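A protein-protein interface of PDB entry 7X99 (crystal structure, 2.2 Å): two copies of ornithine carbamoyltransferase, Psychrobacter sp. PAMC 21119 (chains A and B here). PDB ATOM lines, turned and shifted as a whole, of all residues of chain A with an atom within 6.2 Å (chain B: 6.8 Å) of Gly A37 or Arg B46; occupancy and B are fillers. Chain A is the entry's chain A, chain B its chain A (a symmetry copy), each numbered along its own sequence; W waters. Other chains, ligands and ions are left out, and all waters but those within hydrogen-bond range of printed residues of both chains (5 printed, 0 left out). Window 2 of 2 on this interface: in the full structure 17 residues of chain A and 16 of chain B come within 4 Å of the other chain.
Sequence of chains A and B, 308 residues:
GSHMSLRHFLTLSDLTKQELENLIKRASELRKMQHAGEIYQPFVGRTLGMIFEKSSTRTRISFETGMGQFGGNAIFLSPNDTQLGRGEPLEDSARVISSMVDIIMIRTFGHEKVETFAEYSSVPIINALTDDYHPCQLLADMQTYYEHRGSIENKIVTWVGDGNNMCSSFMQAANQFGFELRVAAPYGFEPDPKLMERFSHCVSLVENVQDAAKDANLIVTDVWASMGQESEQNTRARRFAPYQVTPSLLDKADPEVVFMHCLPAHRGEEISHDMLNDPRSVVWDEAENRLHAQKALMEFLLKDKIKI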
ATOM      1  N   LYS A  32      -4.161  20.280 -12.071  1.00  0.00           N
ATOM      2  CA  LYS A  32      -4.530  21.275 -11.017  1.00  0.00           C
ATOM      3  C   LYS A  32      -5.610  22.230 -11.556  1.00  0.00           C
ATOM      4  O   LYS A  32      -6.562  22.551 -10.828  1.00  0.00           O
ATOM      5  CB  LYS A  32      -3.296  22.081 -10.601  1.00  0.00           C
ATOM      6  CG  LYS A  32      -2.304  21.300  -9.751  1.00  0.00           C
ATOM      7  CD  LYS A  32      -1.090  22.104  -9.335  1.00  0.00           C
ATOM      8  CE  LYS A  32      -0.141  21.353  -8.421  1.00  0.00           C
ATOM      9  NZ  LYS A  32       0.237  20.034  -8.986  1.00  0.00           N
ATOM     10  N   MET A  33      -5.462  22.677 -12.797  1.00  0.00           N
ATOM     11  CA  MET A  33      -6.445  23.566 -13.474  1.00  0.00           C
ATOM     12  C   MET A  33      -7.829  22.915 -13.499  1.00  0.00           C
ATOM     13  O   MET A  33      -8.794  23.555 -13.055  1.00  0.00           O
ATOM     14  CB  MET A  33      -5.988  23.896 -14.892  1.00  0.00           C
ATOM     15  CG  MET A  33      -4.896  24.968 -14.920  1.00  0.00           C
ATOM     16  SD  MET A  33      -3.853  24.883 -16.429  1.00  0.00           S
ATOM     17  CE  MET A  33      -5.046  25.411 -17.659  1.00  0.00           C
ATOM     18  N   GLN A  34      -7.921  21.669 -13.956  1.00  0.00           N
ATOM     19  CA  GLN A  34      -9.229  20.983 -14.083  1.00  0.00           C
ATOM     20  C   GLN A  34      -9.844  20.843 -12.695  1.00  0.00           C
ATOM     21  O   GLN A  34     -11.015  21.151 -12.531  1.00  0.00           O
ATOM     22  CB  GLN A  34      -9.044  19.646 -14.812  1.00  0.00           C
ATOM     23  CG  GLN A  34     -10.344  18.909 -15.084  1.00  0.00           C
ATOM     24  CD  GLN A  34     -11.310  19.678 -15.953  1.00  0.00           C
ATOM     25  OE1 GLN A  34     -10.938  20.474 -16.819  1.00  0.00           O
ATOM     26  NE2 GLN A  34     -12.583  19.446 -15.705  1.00  0.00           N
ATOM     27  N   HIS A  35      -9.092  20.356 -11.722  1.00  0.00           N
ATOM     28  CA  HIS A  35      -9.583  20.163 -10.338  1.00  0.00           C
ATOM     29  C   HIS A  35      -9.983  21.505  -9.707  1.00  0.00           C
ATOM     30  O   HIS A  35     -10.833  21.477  -8.855  1.00  0.00           O
ATOM     31  CB  HIS A  35      -8.528  19.460  -9.464  1.00  0.00           C
ATOM     32  CG  HIS A  35      -8.329  18.017  -9.816  1.00  0.00           C
ATOM     33  ND1 HIS A  35      -7.369  17.234  -9.216  1.00  0.00           N
ATOM     34  CD2 HIS A  35      -8.911  17.228 -10.745  1.00  0.00           C
ATOM     35  CE1 HIS A  35      -7.397  16.016  -9.724  1.00  0.00           C
ATOM     36  NE2 HIS A  35      -8.350  15.973 -10.640  1.00  0.00           N
ATOM     37  N   ALA A  36      -9.318  22.609 -10.033  1.00  0.00           N
ATOM     38  CA  ALA A  36      -9.642  23.958  -9.517  1.00  0.00           C
ATOM     39  C   ALA A  36     -10.830  24.539 -10.289  1.00  0.00           C
ATOM     40  O   ALA A  36     -11.288  25.590  -9.895  1.00  0.00           O
ATOM     41  CB  ALA A  36      -8.444  24.862  -9.661  1.00  0.00           C
ATOM     42  N   GLY A  37     -11.260  23.903 -11.383  1.00  0.00           N
ATOM     43  CA  GLY A  37     -12.479  24.275 -12.117  1.00  0.00           C
ATOM     44  C   GLY A  37     -12.169  25.360 -13.119  1.00  0.00           C
ATOM     45  O   GLY A  37     -13.090  26.015 -13.593  1.00  0.00           O
ATOM     46  N   GLU A  38     -10.899  25.556 -13.436  1.00  0.00           N
ATOM     47  CA  GLU A  38     -10.523  26.474 -14.535  1.00  0.00           C
ATOM     48  C   GLU A  38     -11.008  25.908 -15.874  1.00  0.00           C
ATOM     49  O   GLU A  38     -10.796  24.719 -16.179  1.00  0.00           O
ATOM     50  CB  GLU A  38      -9.030  26.751 -14.589  1.00  0.00           C
ATOM     51  CG  GLU A  38      -8.680  27.610 -15.772  1.00  0.00           C
ATOM     52  CD  GLU A  38      -7.249  28.121 -15.830  1.00  0.00           C
ATOM     53  OE1 GLU A  38      -6.535  27.963 -14.824  1.00  0.00           O
ATOM     54  OE2 GLU A  38      -6.846  28.652 -16.910  1.00  0.00           O
ATOM     55  N   ILE A  39     -11.608  26.774 -16.668  1.00  0.00           N
ATOM     56  CA  ILE A  39     -12.031  26.507 -18.062  1.00  0.00           C
ATOM     57  C   ILE A  39     -10.854  26.877 -18.967  1.00  0.00           C
ATOM     58  O   ILE A  39     -10.383  28.038 -18.954  1.00  0.00           O
ATOM     59  CB  ILE A  39     -13.363  27.213 -18.366  1.00  0.00           C
ATOM     60  CG1 ILE A  39     -14.495  26.567 -17.553  1.00  0.00           C
ATOM     61  CG2 ILE A  39     -13.674  27.179 -19.862  1.00  0.00           C
ATOM     62  CD1 ILE A  39     -15.689  27.484 -17.332  1.00  0.00           C
ATOM     63  N   GLY A  68     -12.962  16.789 -24.988  1.00  0.00           N
ATOM     64  CA  GLY A  68     -14.155  17.485 -24.479  1.00  0.00           C
ATOM     65  C   GLY A  68     -13.798  18.617 -23.520  1.00  0.00           C
ATOM     66  O   GLY A  68     -14.360  19.701 -23.665  1.00  0.00           O
ATOM     67  N   GLN A  69     -12.965  18.358 -22.511  1.00  0.00           N
ATOM     68  CA  GLN A  69     -12.582  19.392 -21.509  1.00  0.00           C
ATOM     69  C   GLN A  69     -11.913  20.555 -22.239  1.00  0.00           C
ATOM     70  O   GLN A  69     -12.110  21.707 -21.813  1.00  0.00           O
ATOM     71  CB  GLN A  69     -11.671  18.820 -20.432  1.00  0.00           C
ATOM     72  CG  GLN A  69     -12.433  18.001 -19.404  1.00  0.00           C
ATOM     73  CD  GLN A  69     -11.486  17.316 -18.448  1.00  0.00           C
ATOM     74  OE1 GLN A  69     -10.265  17.350 -18.606  1.00  0.00           O
ATOM     75  NE2 GLN A  69     -12.053  16.656 -17.466  1.00  0.00           N
ATOM     76  N   PRO B  42     -23.849  25.914 -17.839  1.00  0.00           N
ATOM     77  CA  PRO B  42     -23.115  25.860 -16.580  1.00  0.00           C
ATOM     78  C   PRO B  42     -22.088  24.724 -16.513  1.00  0.00           C
ATOM     79  O   PRO B  42     -21.348  24.703 -15.564  1.00  0.00           O
ATOM     80  CB  PRO B  42     -24.225  25.561 -15.586  1.00  0.00           C
ATOM     81  CG  PRO B  42     -25.165  24.680 -16.364  1.00  0.00           C
ATOM     82  CD  PRO B  42     -25.157  25.252 -17.753  1.00  0.00           C
ATOM     83  N   PHE B  43     -22.065  23.802 -17.489  1.00  0.00           N
ATOM     84  CA  PHE B  43     -21.174  22.616 -17.425  1.00  0.00           C
ATOM     85  C   PHE B  43     -20.112  22.574 -18.516  1.00  0.00           C
ATOM     86  O   PHE B  43     -19.584  21.475 -18.784  1.00  0.00           O
ATOM     87  CB  PHE B  43     -22.048  21.379 -17.461  1.00  0.00           C
ATOM     88  CG  PHE B  43     -22.871  21.264 -16.209  1.00  0.00           C
ATOM     89  CD1 PHE B  43     -22.425  21.822 -15.020  1.00  0.00           C
ATOM     90  CD2 PHE B  43     -24.019  20.505 -16.199  1.00  0.00           C
ATOM     91  CE1 PHE B  43     -23.161  21.668 -13.861  1.00  0.00           C
ATOM     92  CE2 PHE B  43     -24.761  20.371 -15.041  1.00  0.00           C
ATOM     93  CZ  PHE B  43     -24.337  20.968 -13.880  1.00  0.00           C
ATOM     94  N   VAL B  44     -19.740  23.717 -19.079  1.00  0.00           N
ATOM     95  CA  VAL B  44     -18.509  23.792 -19.930  1.00  0.00           C
ATOM     96  C   VAL B  44     -17.361  23.124 -19.150  1.00  0.00           C
ATOM     97  O   VAL B  44     -17.189  23.426 -17.978  1.00  0.00           O
ATOM     98  CB  VAL B  44     -18.150  25.236 -20.352  1.00  0.00           C
ATOM     99  CG1 VAL B  44     -16.970  25.236 -21.336  1.00  0.00           C
ATOM    100  CG2 VAL B  44     -19.324  25.965 -20.992  1.00  0.00           C
ATOM    101  N   GLY B  45     -16.644  22.187 -19.765  1.00  0.00           N
ATOM    102  CA  GLY B  45     -15.488  21.509 -19.151  1.00  0.00           C
ATOM    103  C   GLY B  45     -15.887  20.284 -18.345  1.00  0.00           C
ATOM    104  O   GLY B  45     -14.984  19.668 -17.777  1.00  0.00           O
ATOM    105  N   ARG B  46     -17.189  19.991 -18.244  1.00  0.00           N
ATOM    106  CA  ARG B  46     -17.746  18.913 -17.396  1.00  0.00           C
ATOM    107  C   ARG B  46     -18.167  17.712 -18.269  1.00  0.00           C
ATOM    108  O   ARG B  46     -18.503  17.895 -19.481  1.00  0.00           O
ATOM    109  CB  ARG B  46     -18.898  19.448 -16.547  1.00  0.00           C
ATOM    110  CG  ARG B  46     -18.513  20.618 -15.639  1.00  0.00           C
ATOM    111  CD  ARG B  46     -17.595  20.200 -14.518  1.00  0.00           C
ATOM    112  NE  ARG B  46     -17.137  21.293 -13.656  1.00  0.00           N
ATOM    113  CZ  ARG B  46     -16.123  21.210 -12.786  1.00  0.00           C
ATOM    114  NH1 ARG B  46     -15.769  22.277 -12.105  1.00  0.00           N
ATOM    115  NH2 ARG B  46     -15.434  20.084 -12.623  1.00  0.00           N
ATOM    116  N   THR B  47     -18.134  16.519 -17.671  1.00  0.00           N
ATOM    117  CA  THR B  47     -18.400  15.254 -18.385  1.00  0.00           C
ATOM    118  C   THR B  47     -19.385  14.405 -17.583  1.00  0.00           C
ATOM    119  O   THR B  47     -19.170  14.228 -16.381  1.00  0.00           O
ATOM    120  CB  THR B  47     -17.104  14.491 -18.669  1.00  0.00           C
ATOM    121  OG1 THR B  47     -16.107  15.396 -19.155  1.00  0.00           O
ATOM    122  CG2 THR B  47     -17.301  13.406 -19.702  1.00  0.00           C
ATOM    123  N   LEU B  48     -20.376  13.850 -18.275  1.00  0.00           N
ATOM    124  CA  LEU B  48     -21.293  12.801 -17.768  1.00  0.00           C
ATOM    125  C   LEU B  48     -20.811  11.441 -18.280  1.00  0.00           C
ATOM    126  O   LEU B  48     -20.692  11.254 -19.510  1.00  0.00           O
ATOM    127  CB  LEU B  48     -22.715  13.116 -18.259  1.00  0.00           C
ATOM    128  CG  LEU B  48     -23.748  12.018 -18.027  1.00  0.00           C
ATOM    129  CD1 LEU B  48     -24.050  11.850 -16.560  1.00  0.00           C
ATOM    130  CD2 LEU B  48     -25.001  12.319 -18.786  1.00  0.00           C
ATOM    131  N   MET B  67     -26.801  17.008 -21.266  1.00  0.00           N
ATOM    132  CA  MET B  67     -25.435  17.415 -20.882  1.00  0.00           C
ATOM    133  C   MET B  67     -24.816  18.284 -21.999  1.00  0.00           C
ATOM    134  O   MET B  67     -24.209  19.315 -21.687  1.00  0.00           O
ATOM    135  CB  MET B  67     -24.551  16.196 -20.578  1.00  0.00           C
ATOM    136  CG  MET B  67     -23.180  16.569 -20.067  1.00  0.00           C
ATOM    137  SD  MET B  67     -23.238  17.814 -18.730  1.00  0.00           S
ATOM    138  CE  MET B  67     -22.614  16.863 -17.347  1.00  0.00           C
ATOM    139  N   GLY B  71     -23.461  22.421 -22.192  1.00  0.00           N
ATOM    140  CA  GLY B  71     -22.077  22.738 -22.611  1.00  0.00           C
ATOM    141  C   GLY B  71     -21.095  21.646 -22.213  1.00  0.00           C
ATOM    142  O   GLY B  71     -19.905  21.774 -22.490  1.00  0.00           O
ATOM    143  N   GLY B  72     -21.560  20.568 -21.589  1.00  0.00           N
ATOM    144  CA  GLY B  72     -20.681  19.458 -21.196  1.00  0.00           C
ATOM    145  C   GLY B  72     -20.627  18.399 -22.278  1.00  0.00           C
ATOM    146  O   GLY B  72     -21.102  18.632 -23.361  1.00  0.00           O
ATOM    147  N   ASN B  73     -20.092  17.235 -21.954  1.00  0.00           N
ATOM    148  CA  ASN B  73     -19.971  16.078 -22.869  1.00  0.00           C
ATOM    149  C   ASN B  73     -20.445  14.837 -22.103  1.00  0.00           C
ATOM    150  O   ASN B  73     -20.376  14.827 -20.856  1.00  0.00           O
ATOM    151  CB  ASN B  73     -18.546  15.964 -23.408  1.00  0.00           C
ATOM    152  CG  ASN B  73     -18.246  16.997 -24.475  1.00  0.00           C
ATOM    153  OD1 ASN B  73     -18.759  16.916 -25.577  1.00  0.00           O
ATOM    154  ND2 ASN B  73     -17.424  17.982 -24.157  1.00  0.00           N
ATOM    155  N   ALA B  74     -20.991  13.866 -22.817  1.00  0.00           N
ATOM    156  CA  ALA B  74     -21.479  12.605 -22.238  1.00  0.00           C
ATOM    157  C   ALA B  74     -20.643  11.479 -22.846  1.00  0.00           C
ATOM    158  O   ALA B  74     -20.396  11.532 -24.045  1.00  0.00           O
ATOM    159  CB  ALA B  74     -22.954  12.481 -22.503  1.00  0.00           C
ATOM    160  N   VAL B 101     -14.575  11.826 -14.652  1.00  0.00           N
ATOM    161  CA  VAL B 101     -15.832  12.529 -15.079  1.00  0.00           C
ATOM    162  C   VAL B 101     -16.420  13.263 -13.866  1.00  0.00           C
ATOM    163  O   VAL B 101     -15.870  13.123 -12.788  1.00  0.00           O
ATOM    164  CB  VAL B 101     -16.834  11.546 -15.717  1.00  0.00           C
ATOM    165  CG1 VAL B 101     -16.211  10.789 -16.875  1.00  0.00           C
ATOM    166  CG2 VAL B 101     -17.396  10.573 -14.711  1.00  0.00           C
ATOM    167  N   ASP B 102     -17.495  14.031 -14.030  1.00  0.00           N
ATOM    168  CA  ASP B 102     -17.995  14.930 -12.955  1.00  0.00           C
ATOM    169  C   ASP B 102     -19.305  14.384 -12.370  1.00  0.00           C
ATOM    170  O   ASP B 102     -19.677  14.808 -11.253  1.00  0.00           O
ATOM    171  CB  ASP B 102     -18.104  16.357 -13.495  1.00  0.00           C
ATOM    172  CG  ASP B 102     -16.796  16.813 -14.104  1.00  0.00           C
ATOM    173  OD1 ASP B 102     -15.906  17.169 -13.330  1.00  0.00           O
ATOM    174  OD2 ASP B 102     -16.656  16.755 -15.355  1.00  0.00           O
ATOM    175  N   ILE B 103     -19.972  13.482 -13.095  1.00  0.00           N
ATOM    176  CA  ILE B 103     -21.300  12.917 -12.724  1.00  0.00           C
ATOM    177  C   ILE B 103     -21.468  11.631 -13.518  1.00  0.00           C
ATOM    178  O   ILE B 103     -20.974  11.580 -14.637  1.00  0.00           O
ATOM    179  CB  ILE B 103     -22.416  13.946 -12.983  1.00  0.00           C
ATOM    180  CG1 ILE B 103     -23.801  13.435 -12.540  1.00  0.00           C
ATOM    181  CG2 ILE B 103     -22.381  14.436 -14.420  1.00  0.00           C
ATOM    182  CD1 ILE B 103     -24.798  14.549 -12.104  1.00  0.00           C
ATOM    183  N   LEU B 302     -24.868  18.891  -9.159  1.00  0.00           N
ATOM    184  CA  LEU B 302     -23.573  19.588  -9.391  1.00  0.00           C
ATOM    185  C   LEU B 302     -23.657  21.094  -9.100  1.00  0.00           C
ATOM    186  O   LEU B 302     -22.791  21.842  -9.656  1.00  0.00           O
ATOM    187  CB  LEU B 302     -23.168  19.417 -10.859  1.00  0.00           C
ATOM    188  CG  LEU B 302     -22.769  18.005 -11.262  1.00  0.00           C
ATOM    189  CD1 LEU B 302     -22.267  17.978 -12.704  1.00  0.00           C
ATOM    190  CD2 LEU B 302     -21.745  17.441 -10.296  1.00  0.00           C
ATOM    191  N   LYS B 305     -20.671  23.261  -8.320  1.00  0.00           N
ATOM    192  CA  LYS B 305     -19.777  23.538  -9.475  1.00  0.00           C
ATOM    193  C   LYS B 305     -20.355  24.650 -10.331  1.00  0.00           C
ATOM    194  O   LYS B 305     -19.748  24.951 -11.371  1.00  0.00           O
ATOM    195  CB  LYS B 305     -19.603  22.342 -10.421  1.00  0.00           C
ATOM    196  CG  LYS B 305     -19.244  21.034  -9.744  1.00  0.00           C
ATOM    197  CD  LYS B 305     -18.067  21.150  -8.848  1.00  0.00           C
ATOM    198  CE  LYS B 305     -17.464  19.793  -8.554  1.00  0.00           C
ATOM    199  NZ  LYS B 305     -16.498  19.888  -7.440  1.00  0.00           N
ATOM    200  N   ILE B 306     -21.516  25.185  -9.990  1.00  0.00           N
ATOM    201  CA  ILE B 306     -22.143  26.203 -10.878  1.00  0.00           C
ATOM    202  C   ILE B 306     -21.947  27.609 -10.290  1.00  0.00           C
ATOM    203  O   ILE B 306     -22.473  27.860  -9.177  1.00  0.00           O
ATOM    204  CB  ILE B 306     -23.621  25.925 -11.147  1.00  0.00           C
ATOM    205  CG1 ILE B 306     -23.810  24.562 -11.806  1.00  0.00           C
ATOM    206  CG2 ILE B 306     -24.181  27.061 -12.005  1.00  0.00           C
ATOM    207  CD1 ILE B 306     -25.258  24.203 -12.011  1.00  0.00           C
HETATM  208  O   HOH W   1     -14.833  16.787 -17.297  1.00  0.00           O
HETATM  209  O   HOH W   2     -13.454  17.441 -13.798  1.00  0.00           O
HETATM  210  O   HOH W   3     -17.133  21.161 -22.294  1.00  0.00           O
HETATM  211  O   HOH W   4     -16.488  18.514 -21.176  1.00  0.00           O
HETATM  212  O   HOH W   5     -15.238  16.033 -21.541  1.00  0.00           O
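Among the printed residues, pairs that only touch across the chains: Gly A68 with Asn B73 (3.3 Å), Gln A69 with Gly B45 (3.5 Å) and Gly A37 with Arg B46 (3.8 Å).
The backbone NH (N) of Leu B48 is in hydrogen-bond range of the backbone carbonyl oxygen (O) of Asn B73, 2.8 Å away.
NE2 of Gln A69 lies close to NE2 of Gln A34.
The side-chain carboxylate (OD1) of Asp B102 is in salt-bridge range of the guanidinium group (NH2) of Arg B46 (3.0 Å).
The backbone carbonyl oxygen of Arg B46 sits at hydrogen-bond distance from the backbone NH of Asn B73, 3.0 Å away.
O of Gly B45 is in hydrogen-bond range of NE2 of Gln A34 (3.2 Å).
Gly A37 touches just one residue of chain B: Arg B46 (3.8 Å).
Printed residues of chain B within 4 Å of Gly A68: Asn B73.
Of the printed residues of chain B, Gln A34 touches Gly B45.
Printed residues of chain A within 4 Å of Asn B73: Gly A68 (3.3 Å).
Of the printed residues of chain B, Gln A69 touches Gly B45 (3.5 Å).
Of the printed residues of chain A, Gly B45 touches Gln A34 (3.2 Å) and Gln A69 (3.5 Å).
The nearest residue of chain B that does not touch Gly A37 is Val B44 (6.5 Å).
Water W2 bridges the side-chain carboxylate (OD1) of Asp B102 (2.5 Å) and the side-chain amide nitrogen (NE2) of Gln A34 (2.9 Å).
Water W5 bridges OG1 of Thr B47 and N of Gln A69.
Water W1 lies within hydrogen-bond range of OG1 of Thr B47 (2.6 Å), OD2 of Asp B102 (2.7 Å), NE2 of Gln A69 (2.8 Å) and O of Gly B45 (2.9 Å).
Water W4 lies within hydrogen-bond range of the backbone carbonyl oxygen (O) of Arg B46 (2.7 Å), the side-chain amide nitrogen (ND2) of Asn B73 (3.2 Å) and the backbone carbonyl oxygen (O) of Gly A68 (3.5 Å).
Water W3 lies within hydrogen-bond range of N of Gly B45 (2.8 Å), O of Gly B71 (2.8 Å) and O of Gly A68 (3.4 Å).
No position is printed for both chains.
Of the 4 pairs that touch across the chains among the printed residues, none has its exchanged pair printed and touching as well.
Along chain B the printed residues that touch a printed residue of chain A span positions 45 to 73.
Among the printed residues, 4 pairs touch across the chains.
Among the printed residues, no Asp or Glu carboxylate lies within 4 Å of a Lys or Arg side-chain nitrogen of the other chain.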
